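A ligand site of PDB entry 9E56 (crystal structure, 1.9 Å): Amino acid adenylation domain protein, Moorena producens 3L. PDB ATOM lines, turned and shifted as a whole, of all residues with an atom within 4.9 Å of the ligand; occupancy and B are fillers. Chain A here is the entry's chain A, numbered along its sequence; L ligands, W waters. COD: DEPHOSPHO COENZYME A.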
ATOM      1  N   TYR A  32      37.144  11.709   9.493  1.00  0.00           N
ATOM      2  CA  TYR A  32      38.368  12.281   8.925  1.00  0.00           C
ATOM      3  C   TYR A  32      38.526  13.677   9.506  1.00  0.00           C
ATOM      4  O   TYR A  32      37.673  14.159  10.254  1.00  0.00           O
ATOM      5  CB  TYR A  32      38.307  12.288   7.390  1.00  0.00           C
ATOM      6  CG  TYR A  32      37.000  12.841   6.855  1.00  0.00           C
ATOM      7  CD1 TYR A  32      36.840  14.212   6.622  1.00  0.00           C
ATOM      8  CD2 TYR A  32      35.923  12.002   6.610  1.00  0.00           C
ATOM      9  CE1 TYR A  32      35.642  14.723   6.156  1.00  0.00           C
ATOM     10  CE2 TYR A  32      34.707  12.514   6.134  1.00  0.00           C
ATOM     11  CZ  TYR A  32      34.578  13.865   5.907  1.00  0.00           C
ATOM     12  OH  TYR A  32      33.377  14.363   5.444  1.00  0.00           O
ATOM     13  N   LEU A 110      30.370   4.581   7.635  1.00  0.00           N
ATOM     14  CA  LEU A 110      31.155   5.527   6.858  1.00  0.00           C
ATOM     15  C   LEU A 110      30.492   6.898   6.997  1.00  0.00           C
ATOM     16  O   LEU A 110      29.494   7.180   6.331  1.00  0.00           O
ATOM     17  CB  LEU A 110      31.223   5.071   5.399  1.00  0.00           C
ATOM     18  CG  LEU A 110      31.575   3.594   5.184  1.00  0.00           C
ATOM     19  CD1 LEU A 110      31.344   3.183   3.740  1.00  0.00           C
ATOM     20  CD2 LEU A 110      33.034   3.325   5.568  1.00  0.00           C
ATOM     21  N   THR A 111      31.044   7.732   7.865  1.00  0.00           N
ATOM     22  CA  THR A 111      30.387   8.993   8.179  1.00  0.00           C
ATOM     23  C   THR A 111      30.808  10.085   7.185  1.00  0.00           C
ATOM     24  O   THR A 111      31.718   9.902   6.370  1.00  0.00           O
ATOM     25  CB  THR A 111      30.685   9.449   9.613  1.00  0.00           C
ATOM     26  OG1 THR A 111      32.048   9.906   9.735  1.00  0.00           O
ATOM     27  CG2 THR A 111      30.437   8.322  10.626  1.00  0.00           C
ATOM     28  N   GLY A 112      30.134  11.230   7.264  1.00  0.00           N
ATOM     29  CA  GLY A 112      30.535  12.369   6.463  1.00  0.00           C
ATOM     30  C   GLY A 112      30.395  12.092   4.976  1.00  0.00           C
ATOM     31  O   GLY A 112      29.470  11.411   4.512  1.00  0.00           O
ATOM     32  N   LEU A 113      31.338  12.636   4.212  1.00  0.00           N
ATOM     33  CA  LEU A 113      31.378  12.475   2.766  1.00  0.00           C
ATOM     34  C   LEU A 113      32.142  11.229   2.313  1.00  0.00           C
ATOM     35  O   LEU A 113      32.396  11.099   1.117  1.00  0.00           O
ATOM     36  CB  LEU A 113      31.995  13.726   2.121  1.00  0.00           C
ATOM     37  CG  LEU A 113      31.140  14.992   2.259  1.00  0.00           C
ATOM     38  CD1 LEU A 113      31.889  16.226   1.783  1.00  0.00           C
ATOM     39  CD2 LEU A 113      29.827  14.821   1.476  1.00  0.00           C
ATOM     40  N   SER A 116      29.911   9.587  -0.285  1.00  0.00           N
ATOM     41  CA  SER A 116      29.885  10.413  -1.493  1.00  0.00           C
ATOM     42  C   SER A 116      31.163  10.277  -2.313  1.00  0.00           C
ATOM     43  O   SER A 116      31.119  10.373  -3.536  1.00  0.00           O
ATOM     44  CB  SER A 116      29.636  11.873  -1.101  1.00  0.00           C
ATOM     45  OG  SER A 116      29.624  12.720  -2.232  1.00  0.00           O
ATOM     46  N   TYR A 120      29.407   5.516  -2.713  1.00  0.00           N
ATOM     47  CA  TYR A 120      28.496   5.167  -1.612  1.00  0.00           C
ATOM     48  C   TYR A 120      28.815   3.795  -1.022  1.00  0.00           C
ATOM     49  O   TYR A 120      27.917   3.019  -0.665  1.00  0.00           O
ATOM     50  CB  TYR A 120      27.040   5.282  -2.054  1.00  0.00           C
ATOM     51  CG  TYR A 120      26.808   6.687  -2.554  1.00  0.00           C
ATOM     52  CD1 TYR A 120      26.570   7.736  -1.653  1.00  0.00           C
ATOM     53  CD2 TYR A 120      26.907   6.994  -3.900  1.00  0.00           C
ATOM     54  CE1 TYR A 120      26.401   9.024  -2.094  1.00  0.00           C
ATOM     55  CE2 TYR A 120      26.741   8.274  -4.345  1.00  0.00           C
ATOM     56  CZ  TYR A 120      26.489   9.296  -3.444  1.00  0.00           C
ATOM     57  OH  TYR A 120      26.326  10.577  -3.913  1.00  0.00           O
ATOM     58  N   THR A 139      26.756   2.715   4.948  1.00  0.00           N
ATOM     59  CA  THR A 139      26.697   4.164   4.925  1.00  0.00           C
ATOM     60  C   THR A 139      25.871   4.702   6.079  1.00  0.00           C
ATOM     61  O   THR A 139      26.040   5.864   6.446  1.00  0.00           O
ATOM     62  CB  THR A 139      26.103   4.688   3.606  1.00  0.00           C
ATOM     63  OG1 THR A 139      24.743   4.249   3.498  1.00  0.00           O
ATOM     64  CG2 THR A 139      26.895   4.214   2.377  1.00  0.00           C
ATOM     65  N   HIS A 141      22.913   5.547   6.028  1.00  0.00           N
ATOM     66  CA  HIS A 141      22.088   6.681   5.597  1.00  0.00           C
ATOM     67  C   HIS A 141      20.591   6.455   5.798  1.00  0.00           C
ATOM     68  O   HIS A 141      19.841   7.443   5.834  1.00  0.00           O
ATOM     69  CB  HIS A 141      22.356   7.033   4.130  1.00  0.00           C
ATOM     70  CG  HIS A 141      23.631   7.771   3.919  1.00  0.00           C
ATOM     71  ND1 HIS A 141      24.010   8.272   2.688  1.00  0.00           N
ATOM     72  CD2 HIS A 141      24.618   8.123   4.776  1.00  0.00           C
ATOM     73  CE1 HIS A 141      25.167   8.889   2.799  1.00  0.00           C
ATOM     74  NE2 HIS A 141      25.577   8.798   4.054  1.00  0.00           N
ATOM     75  N   THR A 144      20.384   7.832   9.287  1.00  0.00           N
ATOM     76  CA  THR A 144      20.471   9.276   9.097  1.00  0.00           C
ATOM     77  C   THR A 144      19.150   9.849   8.607  1.00  0.00           C
ATOM     78  O   THR A 144      18.666  10.871   9.117  1.00  0.00           O
ATOM     79  CB  THR A 144      21.582   9.606   8.109  1.00  0.00           C
ATOM     80  OG1 THR A 144      22.834   9.140   8.626  1.00  0.00           O
ATOM     81  CG2 THR A 144      21.663  11.103   7.855  1.00  0.00           C
ATOM     82  N   ILE A 171      16.994  21.112  -0.029  1.00  0.00           N
ATOM     83  CA  ILE A 171      18.238  21.586  -0.621  1.00  0.00           C
ATOM     84  C   ILE A 171      19.235  20.443  -0.615  1.00  0.00           C
ATOM     85  O   ILE A 171      19.833  20.128   0.424  1.00  0.00           O
ATOM     86  CB  ILE A 171      18.799  22.801   0.110  1.00  0.00           C
ATOM     87  CG1 ILE A 171      17.751  23.903   0.206  1.00  0.00           C
ATOM     88  CG2 ILE A 171      20.020  23.311  -0.635  1.00  0.00           C
ATOM     89  CD1 ILE A 171      18.287  25.163   0.925  1.00  0.00           C
ATOM     90  N   GLY A 172      19.452  19.827  -1.774  1.00  0.00           N
ATOM     91  CA  GLY A 172      20.389  18.714  -1.880  1.00  0.00           C
ATOM     92  C   GLY A 172      19.683  17.372  -1.854  1.00  0.00           C
ATOM     93  O   GLY A 172      19.240  16.901  -0.806  1.00  0.00           O
ATOM     94  N   LEU A 173      19.563  16.745  -3.016  1.00  0.00           N
ATOM     95  CA  LEU A 173      18.797  15.519  -3.114  1.00  0.00           C
ATOM     96  C   LEU A 173      19.700  14.372  -3.535  1.00  0.00           C
ATOM     97  O   LEU A 173      19.464  13.719  -4.545  1.00  0.00           O
ATOM     98  CB  LEU A 173      17.614  15.713  -4.062  1.00  0.00           C
ATOM     99  CG  LEU A 173      16.527  16.548  -3.380  1.00  0.00           C
ATOM    100  CD1 LEU A 173      15.611  17.237  -4.361  1.00  0.00           C
ATOM    101  CD2 LEU A 173      15.733  15.685  -2.405  1.00  0.00           C
ATOM    102  N   GLY A 174      20.748  14.158  -2.753  1.00  0.00           N
ATOM    103  CA  GLY A 174      21.676  13.069  -2.958  1.00  0.00           C
ATOM    104  C   GLY A 174      21.284  11.879  -2.119  1.00  0.00           C
ATOM    105  O   GLY A 174      20.087  11.645  -1.894  1.00  0.00           O
ATOM    106  N   SER A 175      22.265  11.128  -1.623  1.00  0.00           N
ATOM    107  CA  SER A 175      21.963   9.903  -0.898  1.00  0.00           C
ATOM    108  C   SER A 175      21.128  10.198   0.348  1.00  0.00           C
ATOM    109  O   SER A 175      20.057   9.587   0.542  1.00  0.00           O
ATOM    110  CB  SER A 175      23.247   9.180  -0.515  1.00  0.00           C
ATOM    111  OG  SER A 175      22.960   8.044   0.291  1.00  0.00           O
ATOM    112  N   VAL A 176      21.579  11.120   1.198  1.00  0.00           N
ATOM    113  CA  VAL A 176      20.821  11.416   2.412  1.00  0.00           C
ATOM    114  C   VAL A 176      19.489  12.074   2.066  1.00  0.00           C
ATOM    115  O   VAL A 176      18.426  11.661   2.555  1.00  0.00           O
ATOM    116  CB  VAL A 176      21.637  12.294   3.369  1.00  0.00           C
ATOM    117  CG1 VAL A 176      20.766  12.769   4.534  1.00  0.00           C
ATOM    118  CG2 VAL A 176      22.848  11.519   3.887  1.00  0.00           C
ATOM    119  N   GLY A 177      19.518  13.089   1.192  1.00  0.00           N
ATOM    120  CA  GLY A 177      18.295  13.824   0.884  1.00  0.00           C
ATOM    121  C   GLY A 177      17.175  12.934   0.376  1.00  0.00           C
ATOM    122  O   GLY A 177      16.009  13.121   0.760  1.00  0.00           O
ATOM    123  N   CYS A 197      15.378  21.282  -4.718  1.00  0.00           N
ATOM    124  CA  CYS A 197      16.467  22.156  -5.133  1.00  0.00           C
ATOM    125  C   CYS A 197      17.766  21.380  -5.209  1.00  0.00           C
ATOM    126  O   CYS A 197      18.189  20.771  -4.216  1.00  0.00           O
ATOM    127  CB  CYS A 197      16.594  23.342  -4.168  1.00  0.00           C
ATOM    128  SG  CYS A 197      18.032  24.360  -4.470  1.00  0.00           S
ATOM    129  N   ASP A 198      18.400  21.389  -6.384  1.00  0.00           N
ATOM    130  CA  ASP A 198      19.722  20.803  -6.578  1.00  0.00           C
ATOM    131  C   ASP A 198      20.334  21.501  -7.790  1.00  0.00           C
ATOM    132  O   ASP A 198      19.749  22.436  -8.347  1.00  0.00           O
ATOM    133  CB  ASP A 198      19.634  19.284  -6.763  1.00  0.00           C
ATOM    134  CG  ASP A 198      20.873  18.538  -6.288  1.00  0.00           C
ATOM    135  OD1 ASP A 198      21.999  18.851  -6.776  1.00  0.00           O
ATOM    136  OD2 ASP A 198      20.747  17.641  -5.400  1.00  0.00           O
ATOM    137  N   VAL A 199      21.514  21.047  -8.204  1.00  0.00           N
ATOM    138  CA  VAL A 199      22.257  21.781  -9.242  1.00  0.00           C
ATOM    139  C   VAL A 199      21.636  21.530 -10.625  1.00  0.00           C
ATOM    140  O   VAL A 199      20.849  20.607 -10.835  1.00  0.00           O
ATOM    141  CB  VAL A 199      23.749  21.412  -9.214  1.00  0.00           C
ATOM    142  CG1 VAL A 199      24.392  21.910  -7.925  1.00  0.00           C
ATOM    143  CG2 VAL A 199      23.937  19.902  -9.352  1.00  0.00           C
ATOM    144  N   LYS A 202      21.332  18.192 -12.501  1.00  0.00           N
ATOM    145  CA  LYS A 202      20.426  17.160 -11.979  1.00  0.00           C
ATOM    146  C   LYS A 202      18.961  17.439 -12.293  1.00  0.00           C
ATOM    147  O   LYS A 202      18.072  16.848 -11.660  1.00  0.00           O
ATOM    148  CB  LYS A 202      20.633  16.995 -10.468  1.00  0.00           C
ATOM    149  CG  LYS A 202      21.986  16.450 -10.088  1.00  0.00           C
ATOM    150  CD  LYS A 202      22.012  15.815  -8.687  1.00  0.00           C
ATOM    151  CE  LYS A 202      23.372  15.151  -8.408  1.00  0.00           C
ATOM    152  NZ  LYS A 202      23.455  14.447  -7.071  1.00  0.00           N
ATOM    153  N   SER A 228      19.920  25.313  -8.548  1.00  0.00           N
ATOM    154  CA  SER A 228      20.992  26.139  -8.004  1.00  0.00           C
ATOM    155  C   SER A 228      22.132  26.263  -9.000  1.00  0.00           C
ATOM    156  O   SER A 228      22.366  25.380  -9.821  1.00  0.00           O
ATOM    157  CB  SER A 228      21.521  25.550  -6.701  1.00  0.00           C
ATOM    158  OG  SER A 228      20.504  25.558  -5.704  1.00  0.00           O
ATOM    159  N   LYS A 229      22.846  27.396  -8.902  1.00  0.00           N
ATOM    160  CA  LYS A 229      24.131  27.555  -9.552  1.00  0.00           C
ATOM    161  C   LYS A 229      25.162  27.653  -8.441  1.00  0.00           C
ATOM    162  O   LYS A 229      25.467  26.628  -7.795  1.00  0.00           O
ATOM    163  CB  LYS A 229      24.120  28.767 -10.497  1.00  0.00           C
ATOM    164  CG  LYS A 229      22.976  28.785 -11.508  1.00  0.00           C
ATOM    165  CD  LYS A 229      22.985  30.075 -12.323  1.00  0.00           C
ATOM    166  CE  LYS A 229      21.719  30.260 -13.154  1.00  0.00           C
ATOM    167  NZ  LYS A 229      21.639  31.624 -13.773  1.00  0.00           N
ATOM    168  N   THR A 230      25.709  28.826  -8.138  1.00  0.00           N
ATOM    169  CA  THR A 230      26.615  28.953  -7.008  1.00  0.00           C
ATOM    170  C   THR A 230      25.880  29.102  -5.671  1.00  0.00           C
ATOM    171  O   THR A 230      26.486  28.862  -4.619  1.00  0.00           O
ATOM    172  CB  THR A 230      27.581  30.126  -7.210  1.00  0.00           C
ATOM    173  OG1 THR A 230      26.873  31.377  -7.084  1.00  0.00           O
ATOM    174  CG2 THR A 230      28.214  30.072  -8.603  1.00  0.00           C
ATOM    175  N   THR A 231      24.605  29.484  -5.689  1.00  0.00           N
ATOM    176  CA  THR A 231      23.766  29.509  -4.500  1.00  0.00           C
ATOM    177  C   THR A 231      22.367  29.065  -4.893  1.00  0.00           C
ATOM    178  O   THR A 231      22.048  28.899  -6.070  1.00  0.00           O
ATOM    179  CB  THR A 231      23.696  30.887  -3.832  1.00  0.00           C
ATOM    180  OG1 THR A 231      23.201  31.861  -4.767  1.00  0.00           O
ATOM    181  CG2 THR A 231      25.056  31.318  -3.296  1.00  0.00           C
ATOM    182  N   VAL A 232      21.510  28.913  -3.885  1.00  0.00           N
ATOM    183  CA  VAL A 232      20.112  28.527  -4.118  1.00  0.00           C
ATOM    184  C   VAL A 232      19.412  29.672  -4.854  1.00  0.00           C
ATOM    185  O   VAL A 232      19.772  30.836  -4.649  1.00  0.00           O
ATOM    186  CB  VAL A 232      19.382  28.189  -2.814  1.00  0.00           C
ATOM    187  CG1 VAL A 232      19.980  26.939  -2.170  1.00  0.00           C
ATOM    188  CG2 VAL A 232      19.416  29.385  -1.847  1.00  0.00           C
ATOM    189  N   ALA A 245      20.791  18.860   2.840  1.00  0.00           N
ATOM    190  CA  ALA A 245      21.701  17.734   2.816  1.00  0.00           C
ATOM    191  C   ALA A 245      22.653  17.895   1.631  1.00  0.00           C
ATOM    192  O   ALA A 245      22.702  17.070   0.716  1.00  0.00           O
ATOM    193  CB  ALA A 245      20.924  16.421   2.749  1.00  0.00           C
ATOM    194  N   THR A 246      23.433  18.975   1.614  1.00  0.00           N
ATOM    195  CA  THR A 246      24.316  19.267   0.498  1.00  0.00           C
ATOM    196  C   THR A 246      25.743  18.837   0.824  1.00  0.00           C
ATOM    197  O   THR A 246      26.110  18.644   1.986  1.00  0.00           O
ATOM    198  CB  THR A 246      24.321  20.754   0.135  1.00  0.00           C
ATOM    199  OG1 THR A 246      25.057  21.465   1.135  1.00  0.00           O
ATOM    200  CG2 THR A 246      22.908  21.311   0.091  1.00  0.00           C
ATOM    201  N   ASN A 247      26.549  18.687  -0.224  1.00  0.00           N
ATOM    202  CA  ASN A 247      27.987  18.549  -0.065  1.00  0.00           C
ATOM    203  C   ASN A 247      28.720  19.856  -0.354  1.00  0.00           C
ATOM    204  O   ASN A 247      29.934  19.838  -0.570  1.00  0.00           O
ATOM    205  CB  ASN A 247      28.508  17.408  -0.941  1.00  0.00           C
ATOM    206  CG  ASN A 247      28.365  17.692  -2.429  1.00  0.00           C
ATOM    207  OD1 ASN A 247      27.484  18.424  -2.860  1.00  0.00           O
ATOM    208  ND2 ASN A 247      29.244  17.106  -3.229  1.00  0.00           N
ATOM    209  N   VAL A 248      28.007  20.994  -0.347  1.00  0.00           N
ATOM    210  CA  VAL A 248      28.581  22.312  -0.621  1.00  0.00           C
ATOM    211  C   VAL A 248      28.096  23.283   0.451  1.00  0.00           C
ATOM    212  O   VAL A 248      26.893  23.493   0.609  1.00  0.00           O
ATOM    213  CB  VAL A 248      28.206  22.811  -2.035  1.00  0.00           C
ATOM    214  CG1 VAL A 248      28.826  24.215  -2.320  1.00  0.00           C
ATOM    215  CG2 VAL A 248      28.692  21.821  -3.091  1.00  0.00           C
ATOM    216  N   VAL A 251      25.393  27.631   0.660  1.00  0.00           N
ATOM    217  CA  VAL A 251      24.623  27.927  -0.541  1.00  0.00           C
ATOM    218  C   VAL A 251      23.310  28.621  -0.215  1.00  0.00           C
ATOM    219  O   VAL A 251      22.633  29.105  -1.126  1.00  0.00           O
ATOM    220  CB  VAL A 251      24.352  26.650  -1.372  1.00  0.00           C
ATOM    221  CG1 VAL A 251      25.668  26.104  -1.923  1.00  0.00           C
ATOM    222  CG2 VAL A 251      23.646  25.618  -0.520  1.00  0.00           C
ATOM    223  N   ASP A 266      21.442  18.556   7.667  1.00  0.00           N
ATOM    224  CA  ASP A 266      22.489  17.580   7.936  1.00  0.00           C
ATOM    225  C   ASP A 266      23.776  17.884   7.179  1.00  0.00           C
ATOM    226  O   ASP A 266      24.748  17.136   7.320  1.00  0.00           O
ATOM    227  CB  ASP A 266      21.998  16.156   7.613  1.00  0.00           C
ATOM    228  CG  ASP A 266      22.936  15.066   8.171  1.00  0.00           C
ATOM    229  OD1 ASP A 266      23.336  15.154   9.362  1.00  0.00           O
ATOM    230  OD2 ASP A 266      23.271  14.123   7.429  1.00  0.00           O
ATOM    231  N   SER A 267      23.840  18.982   6.409  1.00  0.00           N
ATOM    232  CA  SER A 267      25.076  19.328   5.702  1.00  0.00           C
ATOM    233  C   SER A 267      26.199  19.631   6.679  1.00  0.00           C
ATOM    234  O   SER A 267      25.996  20.243   7.736  1.00  0.00           O
ATOM    235  CB  SER A 267      24.864  20.548   4.782  1.00  0.00           C
ATOM    236  OG  SER A 267      23.698  20.428   3.991  1.00  0.00           O
ATOM    237  N   GLY A 268      27.421  19.228   6.298  1.00  0.00           N
ATOM    238  CA  GLY A 268      28.606  19.436   7.105  1.00  0.00           C
ATOM    239  C   GLY A 268      29.826  19.695   6.221  1.00  0.00           C
ATOM    240  O   GLY A 268      30.354  18.788   5.570  1.00  0.00           O
ATOM    241  N   MET A 332      25.301  10.429  16.838  1.00  0.00           N
ATOM    242  CA  MET A 332      25.054  10.630  15.419  1.00  0.00           C
ATOM    243  C   MET A 332      24.335   9.419  14.834  1.00  0.00           C
ATOM    244  O   MET A 332      24.688   8.267  15.115  1.00  0.00           O
ATOM    245  CB  MET A 332      26.377  10.872  14.712  1.00  0.00           C
ATOM    246  CG  MET A 332      26.284  11.074  13.230  1.00  0.00           C
ATOM    247  SD  MET A 332      27.940  11.093  12.493  1.00  0.00           S
ATOM    248  CE  MET A 332      28.694  12.457  13.363  1.00  0.00           C
ATOM    249  N   CYS A 334      24.178   8.020  11.736  1.00  0.00           N
ATOM    250  CA  CYS A 334      24.830   7.036  10.910  1.00  0.00           C
ATOM    251  C   CYS A 334      25.874   6.212  11.723  1.00  0.00           C
ATOM    252  O   CYS A 334      26.080   5.041  11.371  1.00  0.00           O
ATOM    253  CB  CYS A 334      25.470   7.591   9.677  1.00  0.00           C
ATOM    254  SG  CYS A 334      26.638   8.793  10.271  1.00  0.00           S
HETATM  255  N1  COD L   1      22.234  23.488  -4.121  1.00  0.00           N
HETATM  256  C2  COD L   1      21.542  22.373  -3.923  1.00  0.00           C
HETATM  257  N3  COD L   1      22.113  21.194  -3.872  1.00  0.00           N
HETATM  258  C4  COD L   1      23.431  21.088  -3.998  1.00  0.00           C
HETATM  259  C5  COD L   1      24.194  22.185  -4.218  1.00  0.00           C
HETATM  260  C6  COD L   1      23.522  23.442  -4.268  1.00  0.00           C
HETATM  261  N7  COD L   1      24.230  24.683  -4.482  1.00  0.00           N
HETATM  262  N8  COD L   1      25.506  21.757  -4.343  1.00  0.00           N
HETATM  263  C9  COD L   1      25.493  20.449  -4.205  1.00  0.00           C
HETATM  264  N10 COD L   1      24.237  19.994  -4.001  1.00  0.00           N
HETATM  265  C11 COD L   1      23.788  18.734  -3.851  1.00  0.00           C
HETATM  266  C12 COD L   1      24.540  17.673  -4.773  1.00  0.00           C
HETATM  267  O13 COD L   1      24.275  17.971  -6.233  1.00  0.00           O
HETATM  268  C14 COD L   1      24.105  16.550  -4.363  1.00  0.00           C
HETATM  269  O15 COD L   1      22.830  16.127  -4.921  1.00  0.00           O
HETATM  270  C16 COD L   1      23.861  16.796  -2.706  1.00  0.00           C
HETATM  271  O17 COD L   1      24.030  18.066  -2.485  1.00  0.00           O
HETATM  272  C18 COD L   1      24.837  15.963  -1.955  1.00  0.00           C
HETATM  273  O19 COD L   1      24.528  14.619  -2.165  1.00  0.00           O
HETATM  274  P20 COD L   1      25.729  13.525  -1.930  1.00  0.00           P
HETATM  275  O21 COD L   1      27.013  13.932  -2.595  1.00  0.00           O
HETATM  276  O22 COD L   1      25.260  12.152  -2.341  1.00  0.00           O
HETATM  277  O23 COD L   1      26.117  13.535  -0.337  1.00  0.00           O
HETATM  278  P24 COD L   1      25.231  12.809   0.844  1.00  0.00           P
HETATM  279  O25 COD L   1      25.953  11.526   1.179  1.00  0.00           O
HETATM  280  O26 COD L   1      23.805  12.653   0.365  1.00  0.00           O
HETATM  281  O27 COD L   1      25.189  13.845   2.118  1.00  0.00           O
HETATM  282  C28 COD L   1      26.102  14.929   2.229  1.00  0.00           C
HETATM  283  C29 COD L   1      26.303  14.983   3.731  1.00  0.00           C
HETATM  284  C30 COD L   1      24.987  15.398   4.386  1.00  0.00           C
HETATM  285  C31 COD L   1      26.607  13.505   4.161  1.00  0.00           C
HETATM  286  C32 COD L   1      27.452  15.934   4.041  1.00  0.00           C
HETATM  287  O33 COD L   1      27.026  17.302   4.232  1.00  0.00           O
HETATM  288  C34 COD L   1      28.421  15.423   5.105  1.00  0.00           C
HETATM  289  O35 COD L   1      29.363  14.827   4.744  1.00  0.00           O
HETATM  290  N36 COD L   1      28.408  15.574   6.562  1.00  0.00           N
HETATM  291  C37 COD L   1      27.440  16.228   7.458  1.00  0.00           C
HETATM  292  C38 COD L   1      27.213  15.302   8.630  1.00  0.00           C
HETATM  293  C39 COD L   1      27.156  13.799   8.220  1.00  0.00           C
HETATM  294  O40 COD L   1      28.106  13.095   8.401  1.00  0.00           O
HETATM  295  N41 COD L   1      25.962  13.290   7.576  1.00  0.00           N
HETATM  296  C42 COD L   1      25.862  11.888   7.149  1.00  0.00           C
HETATM  297  C43 COD L   1      25.508  10.968   8.339  1.00  0.00           C
HETATM  298  S44 COD L   1      27.033  10.030   8.651  1.00  0.00           S
HETATM  299  O   HOH W   1      30.216  14.060   9.681  1.00  0.00           O
HETATM  300  O   HOH W   2      27.821   9.367   5.620  1.00  0.00           O
HETATM  301  O   HOH W   3      26.851  18.390  -7.437  1.00  0.00           O
HETATM  302  O   HOH W   4      28.387  10.889   1.792  1.00  0.00           O
HETATM  303  O   HOH W   5      24.624  13.045  10.666  1.00  0.00           O
HETATM  304  O   HOH W   6      21.805  14.507   0.093  1.00  0.00           O
HETATM  305  O   HOH W   7      31.233  16.567   6.785  1.00  0.00           O
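The backbone NH of Leu 113 is in hydrogen-bond range of an oxygen (O35) of the ligand. O33 of the ligand lies within hydrogen-bond range of O of Thr 246 (2.8 Å). The backbone NH (N) of Gly 112 sits at hydrogen-bond distance from an oxygen (O40) of the ligand. The side-chain hydroxyl of Ser 116 sits at hydrogen-bond distance from an oxygen (O21) of the ligand (2.9 Å). OD2 of Asp 266 sits at hydrogen-bond distance from N41 of the ligand (2.8 Å). OG of Ser 228 sits at hydrogen-bond distance from N1 of the ligand (3.1 Å). N of Gly 268 lies within hydrogen-bond range of O33 of the ligand (2.9 Å). OD1 of Asp 198 lies within hydrogen-bond range of O13 of the ligand (2.5 Å). O17 of the ligand is in hydrogen-bond range of N of Asn 247. An oxygen (O26) of the ligand lies within hydrogen-bond range of the backbone NH of Val 176 (2.8 Å). O22 of the ligand is in hydrogen-bond range of OH of Tyr 120 (2.5 Å). The side-chain sulfur (SG) of Cys 334 is bonded to a sulfur (S44) of the ligand, at 2.1 Å. The side-chain amino group (NZ) of Lys 202 sits at hydrogen-bond distance from an oxygen (O15) of the ligand, 2.8 Å away. OD1 of Asn 247 lies close to O17 of the ligand, 3.5 Å away. The backbone NH (N) of Ser 175 lies within hydrogen-bond range of an oxygen (O26) of the ligand (2.9 Å).
The side-chain hydroxyl of Ser 175 sits at hydrogen-bond distance from a ring nitrogen (ND1) of His 141. The side-chain hydroxyl of Thr 246 sits at hydrogen-bond distance from the backbone carbonyl oxygen of Val 248 (2.8 Å). The side-chain carboxylate (OD2) of Asp 198 sits at hydrogen-bond distance from the backbone NH (N) of Leu 173, at 2.8 Å. OG of Ser 228 lies within hydrogen-bond range of SG of Cys 197, at 3.0 Å. N of Leu 113 is in hydrogen-bond range of OH of Tyr 32 (2.9 Å). N of Val 232 sits at hydrogen-bond distance from O of Val 251 (3.0 Å). N of Ser 228 lies within hydrogen-bond range of O of Asp 198 (2.9 Å). N of His 141 sits close to OG1 of Thr 139, at 3.4 Å.
Thr 111 touches the ligand (CA to S44, 3.5 Å). His 141 touches the ligand (CE1 to O25, 3.2 Å). OG1 of Thr 144 touches C43 of the ligand (3.3 Å). CG2 of Ile 171 touches C2 of the ligand, at 3.7 Å. CA of Gly 172 touches N3 of the ligand, at 3.6 Å. Leu 173 touches the ligand (N to O15, 3.8 Å). Gly 174 touches the ligand (CA to O19, 3.3 Å). Cys 197 touches the ligand (O to C2, 3.7 Å). Val 199 touches the ligand (CG2 to O13, 3.7 Å). Ala 245 touches the ligand. CG2 of Val 248 touches N8 of the ligand (3.4 Å). Val 251 touches the ligand (CG1 to N7, 3.3 Å). Ser 267 touches the ligand (CA to O33, 3.2 Å). Hydrophobic or aromatic side chains that line the ligand: Leu 113, Tyr 120, His 141, Ile 171, Val 176, Val 199, Val 248 and Val 251. Within 4 Å of the ligand: Thr 111, Gly 112, Leu 113, Ser 116, Tyr 120, His 141, Thr 144, Ile 171, Gly 172, Leu 173, Gly 174, Ser 175, Val 176, Cys 197, Asp 198, Val 199, Lys 202, Ser 228, Ala 245, Thr 246, Asn 247, Val 248, Val 251, Asp 266, Ser 267, Gly 268 and Cys 334. The nearest printed residue that does not touch the ligand is Lys 229 (4.04 Å).
Water W4 lies within hydrogen-bond range of an oxygen (O25) of the ligand, the backbone NH of Ser 116 and the backbone carbonyl oxygen of Gly 112. Water W6 lies within hydrogen-bond range of O26 of the ligand (2.7 Å), O of Ala 245 (2.8 Å), N of Gly 177 (2.9 Å) and N of Gly 174 (3.1 Å). Water W7 lies within hydrogen-bond range of the backbone carbonyl oxygen of Gly 268 (2.7 Å), a nitrogen (N36) of the ligand (3.0 Å) and the side-chain hydroxyl of Tyr 32 (3.4 Å). Water W5 bridges the side-chain carboxylate (OD1) of Asp 266 and a nitrogen (N41) of the ligand.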
